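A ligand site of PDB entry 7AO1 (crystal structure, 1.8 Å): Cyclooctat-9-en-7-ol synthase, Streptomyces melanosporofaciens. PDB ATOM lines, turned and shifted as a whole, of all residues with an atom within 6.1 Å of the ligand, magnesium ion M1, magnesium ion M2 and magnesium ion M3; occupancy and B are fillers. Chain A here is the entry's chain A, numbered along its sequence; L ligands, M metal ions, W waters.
The side-chain hydroxyl of Tyr 295 sits at hydrogen-bond distance from an oxygen (O3) of the ligand.
An oxygen (O4) of the ligand is in salt-bridge range of the guanidinium group of Arg 177, 2.7 Å away.
NE of Arg 294 lies within salt-bridge range of O3 of the ligand (2.8 Å).
NH2 of Arg 227 is in salt-bridge range of O3 of the ligand, at 3.3 Å.
A nitrogen (N1) of the ligand sits at hydrogen-bond distance from the backbone carbonyl oxygen of Ile 181 (3.4 Å).
The side-chain amide nitrogen of Asn 220 is in hydrogen-bond range of the side-chain hydroxyl of Tyr 295, at 3.3 Å.
The guanidinium group (NH1) of Arg 227 lies close to the side-chain carboxylate (OE2) of Glu 228.
O of Glu 228 sits at hydrogen-bond distance from N of Gln 233 (2.8 Å).
The side-chain carboxylate (OE1) of Glu 228 lies within hydrogen-bond range of the side-chain amide nitrogen (ND2) of Asn 236, 3.1 Å away.
NH1 of Arg 177 is in salt-bridge range of OD2 of Asp 180.
The guanidinium group (NH2) of Arg 177 is in salt-bridge range of the side-chain carboxylate (OD1) of Asp 221 (3.0 Å).
NH1 of Arg 294 is in salt-bridge range of OD2 of Asp 111 (3.0 Å).
Phe 107 touches the ligand (CE1 to C3, 3.5 Å).
Within 4 Å of the ligand: Phe 107, Asp 110, Arg 177, Ile 181, Asn 220, Ser 224, Arg 227, Glu 228, Arg 294 and Tyr 295.
Of the 22 residues printed, 1 comes within 4 Å of magnesium ion M1.
The nearest printed residue that does not touch magnesium ion M1 is Arg 227 (4.02 Å).
Residues that only touch magnesium ion M2: Arg 177 (3.9 Å).
Within 4 Å of magnesium ion M2: Arg 177, Asn 220, Ser 224 and Glu 228.
The nearest printed residue that does not touch magnesium ion M2 is Asp 221 (4.4 Å).
One residue has an atom within 4 Å of magnesium ion M3: Asp 110.
Magnesium ion M1 is bound by O1 of the ligand (2.1 Å), water W8 (2.1 Å), OD2 of Asp 110 (2.1 Å), O6 of the ligand (2.1 Å), water W3 (2.2 Å) and water W9 (2.3 Å).
Magnesium ion M2 is bound by O2 of the ligand (1.9 Å), water W5 (2.1 Å), OD1 of Asn 220 (2.1 Å), O5 of the ligand (2.1 Å), OE2 of Glu 228 (2.2 Å) and OG of Ser 224 (2.3 Å).
Magnesium ion M3 is bound by O6 of the ligand (2.0 Å), water W7 (2.0 Å), water W6 (2.0 Å), OD1 of Asp 110 (2.1 Å), water W2 (2.1 Å) and water W9 (2.2 Å).
Water W3 lies within hydrogen-bond range of the side-chain carboxylate of Asp 111 (3.0 Å) and the guanidinium group of Arg 227 (3.5 Å).
Water W6 lies within hydrogen-bond range of O4 of the ligand and O of Asp 180.
Water W2 bridges the side-chain carboxylate of Asp 153 (2.7 Å) and the side-chain carboxylate of Asp 180 (3.1 Å).
Water W7 lies within hydrogen-bond range of the side-chain carboxylate (OD2) of Asp 180 and the guanidinium group (NH1) of Arg 177.
Water W1 lies within hydrogen-bond range of O7 of the ligand (2.6 Å), OH of Tyr 295 (2.9 Å) and ND2 of Asn 220 (3.3 Å).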
ATOM      1  N   ASN A 103      -9.943   2.939 -29.001  1.00  0.00           N
ATOM      2  CA  ASN A 103      -8.707   2.446 -28.426  1.00  0.00           C
ATOM      3  C   ASN A 103      -8.371   3.173 -27.122  1.00  0.00           C
ATOM      4  O   ASN A 103      -7.986   2.527 -26.143  1.00  0.00           O
ATOM      5  CB  ASN A 103      -7.563   2.574 -29.430  1.00  0.00           C
ATOM      6  CG  ASN A 103      -6.489   1.554 -29.198  1.00  0.00           C
ATOM      7  OD1 ASN A 103      -5.389   1.896 -28.761  1.00  0.00           O
ATOM      8  ND2 ASN A 103      -6.841   0.271 -29.422  1.00  0.00           N
ATOM      9  N   THR A 106     -10.721   1.999 -24.231  1.00  0.00           N
ATOM     10  CA  THR A 106     -10.419   0.624 -23.796  1.00  0.00           C
ATOM     11  C   THR A 106      -9.018   0.485 -23.175  1.00  0.00           C
ATOM     12  O   THR A 106      -8.792  -0.436 -22.396  1.00  0.00           O
ATOM     13  CB  THR A 106     -10.633  -0.377 -24.964  1.00  0.00           C
ATOM     14  OG1 THR A 106      -9.849  -0.007 -26.106  1.00  0.00           O
ATOM     15  CG2 THR A 106     -12.080  -0.396 -25.364  1.00  0.00           C
ATOM     16  N   PHE A 107      -8.083   1.405 -23.464  1.00  0.00           N
ATOM     17  CA  PHE A 107      -6.850   1.500 -22.678  1.00  0.00           C
ATOM     18  C   PHE A 107      -7.160   1.807 -21.220  1.00  0.00           C
ATOM     19  O   PHE A 107      -6.590   1.204 -20.305  1.00  0.00           O
ATOM     20  CB  PHE A 107      -5.978   2.592 -23.265  1.00  0.00           C
ATOM     21  CG  PHE A 107      -4.711   2.110 -23.867  1.00  0.00           C
ATOM     22  CD1 PHE A 107      -3.738   1.487 -23.075  1.00  0.00           C
ATOM     23  CD2 PHE A 107      -4.455   2.310 -25.206  1.00  0.00           C
ATOM     24  CE1 PHE A 107      -2.584   1.062 -23.628  1.00  0.00           C
ATOM     25  CE2 PHE A 107      -3.282   1.890 -25.764  1.00  0.00           C
ATOM     26  CZ  PHE A 107      -2.345   1.276 -24.979  1.00  0.00           C
ATOM     27  N   ASP A 110      -8.268  -1.223 -19.636  1.00  0.00           N
ATOM     28  CA  ASP A 110      -7.136  -2.125 -19.421  1.00  0.00           C
ATOM     29  C   ASP A 110      -6.360  -1.733 -18.171  1.00  0.00           C
ATOM     30  O   ASP A 110      -5.784  -2.599 -17.495  1.00  0.00           O
ATOM     31  CB  ASP A 110      -6.192  -2.068 -20.660  1.00  0.00           C
ATOM     32  CG  ASP A 110      -5.030  -3.066 -20.594  1.00  0.00           C
ATOM     33  OD1 ASP A 110      -5.258  -4.309 -20.836  1.00  0.00           O
ATOM     34  OD2 ASP A 110      -3.864  -2.626 -20.341  1.00  0.00           O
ATOM     35  N   ASP A 111      -6.338  -0.445 -17.877  1.00  0.00           N
ATOM     36  CA  ASP A 111      -5.563   0.094 -16.758  1.00  0.00           C
ATOM     37  C   ASP A 111      -6.340   0.143 -15.450  1.00  0.00           C
ATOM     38  O   ASP A 111      -5.796   0.611 -14.452  1.00  0.00           O
ATOM     39  CB  ASP A 111      -5.093   1.513 -17.117  1.00  0.00           C
ATOM     40  CG  ASP A 111      -3.819   1.511 -17.893  1.00  0.00           C
ATOM     41  OD1 ASP A 111      -3.161   0.473 -17.920  1.00  0.00           O
ATOM     42  OD2 ASP A 111      -3.466   2.563 -18.474  1.00  0.00           O
ATOM     43  N   PHE A 149     -13.582  -7.316 -26.445  1.00  0.00           N
ATOM     44  CA  PHE A 149     -12.288  -7.041 -25.846  1.00  0.00           C
ATOM     45  C   PHE A 149     -12.423  -6.734 -24.362  1.00  0.00           C
ATOM     46  O   PHE A 149     -11.635  -7.228 -23.540  1.00  0.00           O
ATOM     47  CB  PHE A 149     -11.589  -5.875 -26.549  1.00  0.00           C
ATOM     48  CG  PHE A 149     -10.330  -5.445 -25.853  1.00  0.00           C
ATOM     49  CD1 PHE A 149      -9.154  -6.148 -26.022  1.00  0.00           C
ATOM     50  CD2 PHE A 149     -10.320  -4.335 -25.040  1.00  0.00           C
ATOM     51  CE1 PHE A 149      -7.955  -5.721 -25.398  1.00  0.00           C
ATOM     52  CE2 PHE A 149      -9.155  -3.907 -24.419  1.00  0.00           C
ATOM     53  CZ  PHE A 149      -7.967  -4.578 -24.601  1.00  0.00           C
ATOM     54  N   ASP A 153     -10.847  -8.872 -21.228  1.00  0.00           N
ATOM     55  CA  ASP A 153      -9.939  -8.290 -20.248  1.00  0.00           C
ATOM     56  C   ASP A 153     -10.500  -8.433 -18.829  1.00  0.00           C
ATOM     57  O   ASP A 153      -9.745  -8.624 -17.871  1.00  0.00           O
ATOM     58  CB  ASP A 153      -9.717  -6.816 -20.549  1.00  0.00           C
ATOM     59  CG  ASP A 153      -8.940  -6.141 -19.442  1.00  0.00           C
ATOM     60  OD1 ASP A 153      -7.808  -6.566 -19.197  1.00  0.00           O
ATOM     61  OD2 ASP A 153      -9.475  -5.201 -18.811  1.00  0.00           O
ATOM     62  N   ARG A 177      -3.170 -13.972 -26.735  1.00  0.00           N
ATOM     63  CA  ARG A 177      -2.994 -12.559 -27.017  1.00  0.00           C
ATOM     64  C   ARG A 177      -3.670 -12.087 -28.328  1.00  0.00           C
ATOM     65  O   ARG A 177      -3.894 -10.874 -28.482  1.00  0.00           O
ATOM     66  CB  ARG A 177      -1.501 -12.256 -27.092  1.00  0.00           C
ATOM     67  CG  ARG A 177      -0.850 -12.386 -25.670  1.00  0.00           C
ATOM     68  CD  ARG A 177      -1.369 -11.240 -24.797  1.00  0.00           C
ATOM     69  NE  ARG A 177      -0.280 -10.275 -24.534  1.00  0.00           N
ATOM     70  CZ  ARG A 177      -0.448  -8.970 -24.226  1.00  0.00           C
ATOM     71  NH1 ARG A 177      -1.654  -8.447 -24.101  1.00  0.00           N
ATOM     72  NH2 ARG A 177       0.620  -8.168 -24.079  1.00  0.00           N
ATOM     73  N   ASP A 180      -6.333 -10.880 -26.467  1.00  0.00           N
ATOM     74  CA  ASP A 180      -6.138 -10.123 -25.229  1.00  0.00           C
ATOM     75  C   ASP A 180      -5.381  -8.797 -25.458  1.00  0.00           C
ATOM     76  O   ASP A 180      -5.695  -7.784 -24.812  1.00  0.00           O
ATOM     77  CB  ASP A 180      -5.406 -10.962 -24.199  1.00  0.00           C
ATOM     78  CG  ASP A 180      -4.973 -10.145 -22.977  1.00  0.00           C
ATOM     79  OD1 ASP A 180      -5.823  -9.898 -22.101  1.00  0.00           O
ATOM     80  OD2 ASP A 180      -3.805  -9.686 -22.935  1.00  0.00           O
ATOM     81  N   ILE A 181      -4.410  -8.772 -26.393  1.00  0.00           N
ATOM     82  CA  ILE A 181      -3.694  -7.523 -26.632  1.00  0.00           C
ATOM     83  C   ILE A 181      -4.600  -6.530 -27.341  1.00  0.00           C
ATOM     84  O   ILE A 181      -4.305  -5.332 -27.345  1.00  0.00           O
ATOM     85  CB  ILE A 181      -2.375  -7.747 -27.402  1.00  0.00           C
ATOM     86  CG1 ILE A 181      -1.390  -6.560 -27.165  1.00  0.00           C
ATOM     87  CG2 ILE A 181      -2.649  -7.972 -28.931  1.00  0.00           C
ATOM     88  CD1 ILE A 181       0.000  -6.852 -27.575  1.00  0.00           C
ATOM     89  N   GLY A 182      -5.723  -6.998 -27.915  1.00  0.00           N
ATOM     90  CA  GLY A 182      -6.646  -6.111 -28.608  1.00  0.00           C
ATOM     91  C   GLY A 182      -6.419  -5.993 -30.108  1.00  0.00           C
ATOM     92  O   GLY A 182      -7.050  -5.122 -30.751  1.00  0.00           O
ATOM     93  N   ASN A 220       5.580  -5.124 -27.407  1.00  0.00           N
ATOM     94  CA  ASN A 220       4.931  -4.604 -26.222  1.00  0.00           C
ATOM     95  C   ASN A 220       5.434  -5.308 -24.971  1.00  0.00           C
ATOM     96  O   ASN A 220       5.586  -4.667 -23.933  1.00  0.00           O
ATOM     97  CB  ASN A 220       3.398  -4.752 -26.295  1.00  0.00           C
ATOM     98  CG  ASN A 220       2.714  -4.278 -25.002  1.00  0.00           C
ATOM     99  OD1 ASN A 220       2.442  -5.076 -24.101  1.00  0.00           O
ATOM    100  ND2 ASN A 220       2.470  -2.983 -24.900  1.00  0.00           N
ATOM    101  N   ASP A 221       5.599  -6.636 -25.036  1.00  0.00           N
ATOM    102  CA  ASP A 221       5.944  -7.391 -23.821  1.00  0.00           C
ATOM    103  C   ASP A 221       7.310  -6.947 -23.303  1.00  0.00           C
ATOM    104  O   ASP A 221       7.534  -6.807 -22.089  1.00  0.00           O
ATOM    105  CB  ASP A 221       5.938  -8.881 -24.086  1.00  0.00           C
ATOM    106  CG  ASP A 221       4.508  -9.490 -24.110  1.00  0.00           C
ATOM    107  OD1 ASP A 221       3.510  -8.774 -23.823  1.00  0.00           O
ATOM    108  OD2 ASP A 221       4.415 -10.691 -24.448  1.00  0.00           O
ATOM    109  N   SER A 224       6.871  -3.400 -21.645  1.00  0.00           N
ATOM    110  CA  SER A 224       5.929  -3.263 -20.565  1.00  0.00           C
ATOM    111  C   SER A 224       6.179  -4.313 -19.482  1.00  0.00           C
ATOM    112  O   SER A 224       5.426  -4.364 -18.501  1.00  0.00           O
ATOM    113  CB  SER A 224       4.489  -3.334 -21.089  1.00  0.00           C
ATOM    114  OG  SER A 224       4.141  -4.673 -21.414  1.00  0.00           O
ATOM    115  N   TYR A 225       7.227  -5.127 -19.621  1.00  0.00           N
ATOM    116  CA  TYR A 225       7.570  -6.132 -18.626  1.00  0.00           C
ATOM    117  C   TYR A 225       7.712  -5.529 -17.231  1.00  0.00           C
ATOM    118  O   TYR A 225       7.139  -6.037 -16.262  1.00  0.00           O
ATOM    119  CB  TYR A 225       8.868  -6.835 -19.004  1.00  0.00           C
ATOM    120  CG  TYR A 225       9.306  -7.913 -18.060  1.00  0.00           C
ATOM    121  CD1 TYR A 225       8.803  -9.200 -18.187  1.00  0.00           C
ATOM    122  CD2 TYR A 225      10.266  -7.675 -17.057  1.00  0.00           C
ATOM    123  CE1 TYR A 225       9.196 -10.214 -17.361  1.00  0.00           C
ATOM    124  CE2 TYR A 225      10.671  -8.697 -16.231  1.00  0.00           C
ATOM    125  CZ  TYR A 225      10.129  -9.964 -16.366  1.00  0.00           C
ATOM    126  OH  TYR A 225      10.526 -11.013 -15.552  1.00  0.00           O
ATOM    127  N   ARG A 227       6.760  -2.698 -15.750  1.00  0.00           N
ATOM    128  CA  ARG A 227       5.486  -2.280 -15.180  1.00  0.00           C
ATOM    129  C   ARG A 227       4.631  -3.487 -14.806  1.00  0.00           C
ATOM    130  O   ARG A 227       4.086  -3.556 -13.693  1.00  0.00           O
ATOM    131  CB  ARG A 227       4.730  -1.373 -16.173  1.00  0.00           C
ATOM    132  CG  ARG A 227       3.226  -1.312 -15.922  1.00  0.00           C
ATOM    133  CD  ARG A 227       2.538  -0.107 -16.574  1.00  0.00           C
ATOM    134  NE  ARG A 227       2.767  -0.052 -18.033  1.00  0.00           N
ATOM    135  CZ  ARG A 227       2.110  -0.754 -18.954  1.00  0.00           C
ATOM    136  NH1 ARG A 227       1.106  -1.585 -18.624  1.00  0.00           N
ATOM    137  NH2 ARG A 227       2.446  -0.614 -20.238  1.00  0.00           N
ATOM    138  N   GLU A 228       4.543  -4.480 -15.704  1.00  0.00           N
ATOM    139  CA  GLU A 228       3.605  -5.576 -15.476  1.00  0.00           C
ATOM    140  C   GLU A 228       4.054  -6.483 -14.332  1.00  0.00           C
ATOM    141  O   GLU A 228       3.222  -6.895 -13.508  1.00  0.00           O
ATOM    142  CB  GLU A 228       3.374  -6.362 -16.784  1.00  0.00           C
ATOM    143  CG  GLU A 228       2.444  -5.533 -17.735  1.00  0.00           C
ATOM    144  CD  GLU A 228       2.415  -5.981 -19.183  1.00  0.00           C
ATOM    145  OE1 GLU A 228       3.043  -7.006 -19.539  1.00  0.00           O
ATOM    146  OE2 GLU A 228       1.735  -5.292 -19.940  1.00  0.00           O
ATOM    147  N   GLN A 233       1.016  -8.606 -12.952  1.00  0.00           N
ATOM    148  CA  GLN A 233       0.358  -9.010 -14.203  1.00  0.00           C
ATOM    149  C   GLN A 233       1.179 -10.103 -14.900  1.00  0.00           C
ATOM    150  O   GLN A 233       2.367  -9.922 -15.170  1.00  0.00           O
ATOM    151  CB  GLN A 233       0.167  -7.766 -15.092  1.00  0.00           C
ATOM    152  CG  GLN A 233      -1.027  -6.913 -14.613  1.00  0.00           C
ATOM    153  CD  GLN A 233      -1.089  -5.524 -15.200  1.00  0.00           C
ATOM    154  OE1 GLN A 233      -0.073  -4.864 -15.339  1.00  0.00           O
ATOM    155  NE2 GLN A 233      -2.296  -5.070 -15.545  1.00  0.00           N
ATOM    156  N   THR A 235       0.594 -11.527 -17.975  1.00  0.00           N
ATOM    157  CA  THR A 235       0.391 -11.602 -19.449  1.00  0.00           C
ATOM    158  C   THR A 235       1.584 -10.952 -20.137  1.00  0.00           C
ATOM    159  O   THR A 235       1.571  -9.794 -20.555  1.00  0.00           O
ATOM    160  CB  THR A 235      -0.926 -10.935 -19.849  1.00  0.00           C
ATOM    161  OG1 THR A 235      -1.976 -11.507 -19.088  1.00  0.00           O
ATOM    162  CG2 THR A 235      -1.271 -11.181 -21.346  1.00  0.00           C
ATOM    163  N   ASN A 236       2.651 -11.735 -20.300  1.00  0.00           N
ATOM    164  CA  ASN A 236       3.884 -11.210 -20.893  1.00  0.00           C
ATOM    165  C   ASN A 236       4.808 -12.361 -21.219  1.00  0.00           C
ATOM    166  O   ASN A 236       5.167 -13.127 -20.304  1.00  0.00           O
ATOM    167  CB  ASN A 236       4.579 -10.250 -19.922  1.00  0.00           C
ATOM    168  CG  ASN A 236       5.758  -9.585 -20.537  1.00  0.00           C
ATOM    169  OD1 ASN A 236       6.719 -10.263 -21.010  1.00  0.00           O
ATOM    170  ND2 ASN A 236       5.723  -8.260 -20.574  1.00  0.00           N
ATOM    171  N   ARG A 294       4.448   6.150 -21.581  1.00  0.00           N
ATOM    172  CA  ARG A 294       3.826   4.976 -20.990  1.00  0.00           C
ATOM    173  C   ARG A 294       4.846   3.881 -20.701  1.00  0.00           C
ATOM    174  O   ARG A 294       4.783   3.187 -19.697  1.00  0.00           O
ATOM    175  CB  ARG A 294       2.711   4.464 -21.905  1.00  0.00           C
ATOM    176  CG  ARG A 294       2.036   3.167 -21.402  1.00  0.00           C
ATOM    177  CD  ARG A 294       0.813   2.745 -22.226  1.00  0.00           C
ATOM    178  NE  ARG A 294       0.148   1.545 -21.691  1.00  0.00           N
ATOM    179  CZ  ARG A 294      -0.667   1.539 -20.636  1.00  0.00           C
ATOM    180  NH1 ARG A 294      -0.919   2.675 -19.989  1.00  0.00           N
ATOM    181  NH2 ARG A 294      -1.216   0.392 -20.219  1.00  0.00           N
ATOM    182  N   TYR A 295       5.802   3.697 -21.609  1.00  0.00           N
ATOM    183  CA  TYR A 295       6.782   2.635 -21.440  1.00  0.00           C
ATOM    184  C   TYR A 295       8.114   3.184 -20.937  1.00  0.00           C
ATOM    185  O   TYR A 295       9.108   2.455 -20.941  1.00  0.00           O
ATOM    186  CB  TYR A 295       6.964   1.882 -22.761  1.00  0.00           C
ATOM    187  CG  TYR A 295       5.615   1.424 -23.268  1.00  0.00           C
ATOM    188  CD1 TYR A 295       5.017   0.264 -22.729  1.00  0.00           C
ATOM    189  CD2 TYR A 295       4.923   2.166 -24.179  1.00  0.00           C
ATOM    190  CE1 TYR A 295       3.749  -0.148 -23.139  1.00  0.00           C
ATOM    191  CE2 TYR A 295       3.646   1.767 -24.613  1.00  0.00           C
ATOM    192  CZ  TYR A 295       3.070   0.602 -24.077  1.00  0.00           C
ATOM    193  OH  TYR A 295       1.809   0.189 -24.499  1.00  0.00           O
HETATM  194  C1  LIG L   1      -3.024  -2.949 -24.821  1.00  0.00           C
HETATM  195  C2  LIG L   1      -4.377  -2.294 -24.941  1.00  0.00           C
HETATM  196  C3  LIG L   1      -2.348  -2.464 -23.525  1.00  0.00           C
HETATM  197  C4  LIG L   1      -1.043  -3.237 -23.357  1.00  0.00           C
HETATM  198  O1  LIG L   1      -0.713  -2.336 -20.843  1.00  0.00           O
HETATM  199  P1  LIG L   1       0.075  -2.394 -22.119  1.00  0.00           P
HETATM  200  O2  LIG L   1       1.361  -3.221 -22.016  1.00  0.00           O
HETATM  201  O3  LIG L   1       0.265  -1.031 -22.731  1.00  0.00           O
HETATM  202  P2  LIG L   1      -1.350  -4.972 -22.741  1.00  0.00           P
HETATM  203  O4  LIG L   1      -2.037  -5.757 -23.907  1.00  0.00           O
HETATM  204  O5  LIG L   1      -0.063  -5.618 -22.395  1.00  0.00           O
HETATM  205  O6  LIG L   1      -2.314  -4.979 -21.578  1.00  0.00           O
HETATM  206  O7  LIG L   1      -0.401  -3.329 -24.611  1.00  0.00           O
HETATM  207  N1  LIG L   1      -4.709  -2.151 -26.350  1.00  0.00           N
HETATM  208 MG    MG M   1      -2.079  -3.609 -19.996  1.00  0.00          MG
HETATM  209 MG    MG M   2       1.934  -5.069 -22.078  1.00  0.00          MG
HETATM  210 MG    MG M   3      -4.033  -5.939 -21.214  1.00  0.00          MG
HETATM  211  O   HOH W   1      -0.065  -1.219 -26.156  1.00  0.00           O
HETATM  212  O   HOH W   2      -5.699  -7.132 -20.820  1.00  0.00           O
HETATM  213  O   HOH W   3      -2.252  -2.362 -18.223  1.00  0.00           O
HETATM  214  O   HOH W   4      -0.379  -7.660 -20.694  1.00  0.00           O
HETATM  215  O   HOH W   5       2.586  -7.031 -22.163  1.00  0.00           O
HETATM  216  O   HOH W   6      -4.464  -5.804 -23.210  1.00  0.00           O
HETATM  217  O   HOH W   7      -3.104  -7.715 -21.119  1.00  0.00           O
HETATM  218  O   HOH W   8      -0.512  -4.450 -18.963  1.00  0.00           O
HETATM  219  O   HOH W   9      -3.318  -5.383 -19.231  1.00  0.00           O
